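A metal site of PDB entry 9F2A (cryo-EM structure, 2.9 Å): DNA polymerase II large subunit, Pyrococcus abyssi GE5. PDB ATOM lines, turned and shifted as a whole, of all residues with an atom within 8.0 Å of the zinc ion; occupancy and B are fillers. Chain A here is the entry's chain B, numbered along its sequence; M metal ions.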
ATOM      1  N   LYS A 705      28.491  -8.350  13.850  1.00  0.00           N
ATOM      2  CA  LYS A 705      28.554  -9.300  12.744  1.00  0.00           C
ATOM      3  C   LYS A 705      27.774  -8.767  11.548  1.00  0.00           C
ATOM      4  O   LYS A 705      26.630  -8.343  11.683  1.00  0.00           O
ATOM      5  CB  LYS A 705      27.990 -10.658  13.157  1.00  0.00           C
ATOM      6  CG  LYS A 705      28.127 -11.737  12.114  1.00  0.00           C
ATOM      7  CD  LYS A 705      27.671 -13.076  12.645  1.00  0.00           C
ATOM      8  CE  LYS A 705      27.907 -14.185  11.642  1.00  0.00           C
ATOM      9  NZ  LYS A 705      29.343 -14.276  11.259  1.00  0.00           N
ATOM     10  N   CYS A 706      28.413  -8.802  10.382  1.00  0.00           N
ATOM     11  CA  CYS A 706      27.785  -8.337   9.140  1.00  0.00           C
ATOM     12  C   CYS A 706      26.811  -9.398   8.617  1.00  0.00           C
ATOM     13  O   CYS A 706      27.186 -10.571   8.529  1.00  0.00           O
ATOM     14  CB  CYS A 706      28.844  -8.020   8.089  1.00  0.00           C
ATOM     15  SG  CYS A 706      28.204  -7.518   6.463  1.00  0.00           S
ATOM     16  N   PRO A 707      25.586  -9.022   8.275  1.00  0.00           N
ATOM     17  CA  PRO A 707      24.604 -10.036   7.839  1.00  0.00           C
ATOM     18  C   PRO A 707      24.993 -10.786   6.580  1.00  0.00           C
ATOM     19  O   PRO A 707      24.627 -11.956   6.437  1.00  0.00           O
ATOM     20  CB  PRO A 707      23.325  -9.222   7.631  1.00  0.00           C
ATOM     21  CG  PRO A 707      23.541  -7.943   8.360  1.00  0.00           C
ATOM     22  CD  PRO A 707      25.003  -7.670   8.287  1.00  0.00           C
ATOM     23  N   LYS A 708      25.724 -10.155   5.667  1.00  0.00           N
ATOM     24  CA  LYS A 708      25.997 -10.753   4.361  1.00  0.00           C
ATOM     25  C   LYS A 708      27.322 -11.517   4.316  1.00  0.00           C
ATOM     26  O   LYS A 708      27.332 -12.704   3.986  1.00  0.00           O
ATOM     27  CB  LYS A 708      25.974  -9.673   3.289  1.00  0.00           C
ATOM     28  CG  LYS A 708      24.578  -9.167   2.962  1.00  0.00           C
ATOM     29  CD  LYS A 708      24.607  -8.122   1.866  1.00  0.00           C
ATOM     30  CE  LYS A 708      25.173  -6.814   2.379  1.00  0.00           C
ATOM     31  NZ  LYS A 708      24.314  -6.242   3.458  1.00  0.00           N
ATOM     32  N   CYS A 709      28.428 -10.859   4.650  1.00  0.00           N
ATOM     33  CA  CYS A 709      29.743 -11.471   4.500  1.00  0.00           C
ATOM     34  C   CYS A 709      30.253 -12.147   5.763  1.00  0.00           C
ATOM     35  O   CYS A 709      31.187 -12.948   5.692  1.00  0.00           O
ATOM     36  CB  CYS A 709      30.774 -10.438   4.048  1.00  0.00           C
ATOM     37  SG  CYS A 709      31.288  -9.289   5.326  1.00  0.00           S
ATOM     38  N   GLY A 710      29.673 -11.850   6.925  1.00  0.00           N
ATOM     39  CA  GLY A 710      30.063 -12.517   8.144  1.00  0.00           C
ATOM     40  C   GLY A 710      31.287 -11.965   8.838  1.00  0.00           C
ATOM     41  O   GLY A 710      31.903 -12.670   9.633  1.00  0.00           O
ATOM     42  N   HIS A 711      31.648 -10.710   8.563  1.00  0.00           N
ATOM     43  CA  HIS A 711      32.782 -10.099   9.244  1.00  0.00           C
ATOM     44  C   HIS A 711      32.447  -9.840  10.706  1.00  0.00           C
ATOM     45  O   HIS A 711      31.340  -9.421  11.031  1.00  0.00           O
ATOM     46  CB  HIS A 711      33.166  -8.794   8.550  1.00  0.00           C
ATOM     47  CG  HIS A 711      34.456  -8.206   9.042  1.00  0.00           C
ATOM     48  ND1 HIS A 711      35.650  -8.896   8.979  1.00  0.00           N
ATOM     49  CD2 HIS A 711      34.733  -7.012   9.598  1.00  0.00           C
ATOM     50  CE1 HIS A 711      36.614  -8.137   9.473  1.00  0.00           C
ATOM     51  NE2 HIS A 711      36.087  -6.996   9.861  1.00  0.00           N
ATOM     52  N   VAL A 712      33.414 -10.106  11.589  1.00  0.00           N
ATOM     53  CA  VAL A 712      33.250  -9.899  13.024  1.00  0.00           C
ATOM     54  C   VAL A 712      34.305  -8.902  13.479  1.00  0.00           C
ATOM     55  O   VAL A 712      35.503  -9.127  13.307  1.00  0.00           O
ATOM     56  CB  VAL A 712      33.368 -11.223  13.796  1.00  0.00           C
ATOM     57  CG1 VAL A 712      33.114 -10.993  15.267  1.00  0.00           C
ATOM     58  CG2 VAL A 712      32.409 -12.248  13.230  1.00  0.00           C
ATOM     59  N   LEU A 717      30.104  -0.269  10.967  1.00  0.00           N
ATOM     60  CA  LEU A 717      29.969  -0.450   9.527  1.00  0.00           C
ATOM     61  C   LEU A 717      30.975  -1.474   9.040  1.00  0.00           C
ATOM     62  O   LEU A 717      32.134  -1.473   9.470  1.00  0.00           O
ATOM     63  CB  LEU A 717      30.157   0.871   8.780  1.00  0.00           C
ATOM     64  CG  LEU A 717      28.939   1.796   8.702  1.00  0.00           C
ATOM     65  CD1 LEU A 717      29.265   3.001   7.845  1.00  0.00           C
ATOM     66  CD2 LEU A 717      27.742   1.060   8.153  1.00  0.00           C
ATOM     67  N   CYS A 718      30.531  -2.339   8.143  1.00  0.00           N
ATOM     68  CA  CYS A 718      31.401  -3.385   7.613  1.00  0.00           C
ATOM     69  C   CYS A 718      32.492  -2.765   6.757  1.00  0.00           C
ATOM     70  O   CYS A 718      32.207  -1.951   5.866  1.00  0.00           O
ATOM     71  CB  CYS A 718      30.579  -4.387   6.799  1.00  0.00           C
ATOM     72  SG  CYS A 718      31.562  -5.623   5.941  1.00  0.00           S
ATOM     73  N   PRO A 719      33.759  -3.122   6.993  1.00  0.00           N
ATOM     74  CA  PRO A 719      34.861  -2.537   6.205  1.00  0.00           C
ATOM     75  C   PRO A 719      34.862  -2.927   4.742  1.00  0.00           C
ATOM     76  O   PRO A 719      35.565  -2.277   3.954  1.00  0.00           O
ATOM     77  CB  PRO A 719      36.109  -3.095   6.917  1.00  0.00           C
ATOM     78  CG  PRO A 719      35.631  -3.469   8.277  1.00  0.00           C
ATOM     79  CD  PRO A 719      34.259  -3.983   8.063  1.00  0.00           C
ATOM     80  N   ASN A 720      34.103  -3.948   4.328  1.00  0.00           N
ATOM     81  CA  ASN A 720      34.114  -4.392   2.945  1.00  0.00           C
ATOM     82  C   ASN A 720      32.807  -4.065   2.229  1.00  0.00           C
ATOM     83  O   ASN A 720      32.823  -3.389   1.198  1.00  0.00           O
ATOM     84  CB  ASN A 720      34.392  -5.904   2.888  1.00  0.00           C
ATOM     85  CG  ASN A 720      35.725  -6.269   3.491  1.00  0.00           C
ATOM     86  OD1 ASN A 720      36.721  -5.567   3.290  1.00  0.00           O
ATOM     87  ND2 ASN A 720      35.756  -7.373   4.234  1.00  0.00           N
ATOM     88  N   CYS A 721      31.661  -4.526   2.754  1.00  0.00           N
ATOM     89  CA  CYS A 721      30.390  -4.248   2.105  1.00  0.00           C
ATOM     90  C   CYS A 721      29.998  -2.783   2.253  1.00  0.00           C
ATOM     91  O   CYS A 721      29.587  -2.134   1.281  1.00  0.00           O
ATOM     92  CB  CYS A 721      29.298  -5.146   2.686  1.00  0.00           C
ATOM     93  SG  CYS A 721      29.736  -6.882   2.893  1.00  0.00           S
ATOM     94  N   GLY A 722      30.112  -2.242   3.458  1.00  0.00           N
ATOM     95  CA  GLY A 722      29.573  -0.947   3.778  1.00  0.00           C
ATOM     96  C   GLY A 722      28.182  -0.969   4.366  1.00  0.00           C
ATOM     97  O   GLY A 722      27.436   0.002   4.172  1.00  0.00           O
ATOM     98  N   THR A 723      27.805  -2.023   5.084  1.00  0.00           N
ATOM     99  CA  THR A 723      26.461  -2.190   5.618  1.00  0.00           C
ATOM    100  C   THR A 723      26.533  -2.352   7.127  1.00  0.00           C
ATOM    101  O   THR A 723      27.510  -2.864   7.661  1.00  0.00           O
ATOM    102  CB  THR A 723      25.759  -3.404   5.003  1.00  0.00           C
ATOM    103  OG1 THR A 723      26.594  -4.562   5.139  1.00  0.00           O
ATOM    104  CG2 THR A 723      25.482  -3.166   3.531  1.00  0.00           C
ATOM    105  N   ARG A 724      25.485  -1.892   7.804  1.00  0.00           N
ATOM    106  CA  ARG A 724      25.481  -1.886   9.263  1.00  0.00           C
ATOM    107  C   ARG A 724      25.415  -3.311   9.811  1.00  0.00           C
ATOM    108  O   ARG A 724      24.714  -4.171   9.271  1.00  0.00           O
ATOM    109  CB  ARG A 724      24.303  -1.057   9.783  1.00  0.00           C
ATOM    110  CG  ARG A 724      24.396  -0.749  11.260  1.00  0.00           C
ATOM    111  CD  ARG A 724      23.511   0.411  11.660  1.00  0.00           C
ATOM    112  NE  ARG A 724      23.240   0.401  13.091  1.00  0.00           N
ATOM    113  CZ  ARG A 724      23.731   1.285  13.955  1.00  0.00           C
ATOM    114  NH1 ARG A 724      24.515   2.267  13.564  1.00  0.00           N
ATOM    115  NH2 ARG A 724      23.412   1.176  15.242  1.00  0.00           N
ATOM    116  N   LYS A 725      26.156  -3.549  10.885  1.00  0.00           N
ATOM    117  CA  LYS A 725      26.296  -4.865  11.491  1.00  0.00           C
ATOM    118  C   LYS A 725      25.385  -4.991  12.711  1.00  0.00           C
ATOM    119  O   LYS A 725      24.813  -4.012  13.208  1.00  0.00           O
ATOM    120  CB  LYS A 725      27.753  -5.114  11.879  1.00  0.00           C
ATOM    121  CG  LYS A 725      28.718  -4.987  10.712  1.00  0.00           C
ATOM    122  CD  LYS A 725      29.988  -5.790  10.929  1.00  0.00           C
ATOM    123  CE  LYS A 725      31.098  -4.935  11.515  1.00  0.00           C
ATOM    124  NZ  LYS A 725      32.236  -5.770  11.984  1.00  0.00           N
HETATM  125 ZN    ZN M   1      30.126  -7.288   5.153  1.00  0.00          ZN
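Of the 17 residues printed, 4 come within 4 Å of the zinc ion.
The zinc ion is bound by the side-chain sulfur (SG) of Cys 709 (2.3 Å), the side-chain sulfur (SG) of Cys 721 (2.3 Å), the side-chain sulfur (SG) of Cys 718 (2.3 Å) and the side-chain sulfur (SG) of Cys 706 (2.3 Å).
The backbone NH (N) of His 711 sits close to the side-chain sulfur (SG) of Cys 709 (3.6 Å). The backbone NH of Cys 718 is in hydrogen-bond range of the backbone carbonyl oxygen of Thr 723 (3.1 Å). The side-chain sulfur of Cys 718 lies close to the backbone NH of Asn 720 (3.4 Å). The side-chain sulfur of Cys 706 lies close to the side-chain hydroxyl of Thr 723 (3.6 Å). The backbone NH of Cys 706 lies within hydrogen-bond range of the backbone carbonyl oxygen of His 711, at 3.1 Å. The side-chain sulfur (SG) of Cys 706 lies close to the backbone NH (N) of Lys 708 (3.7 Å).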
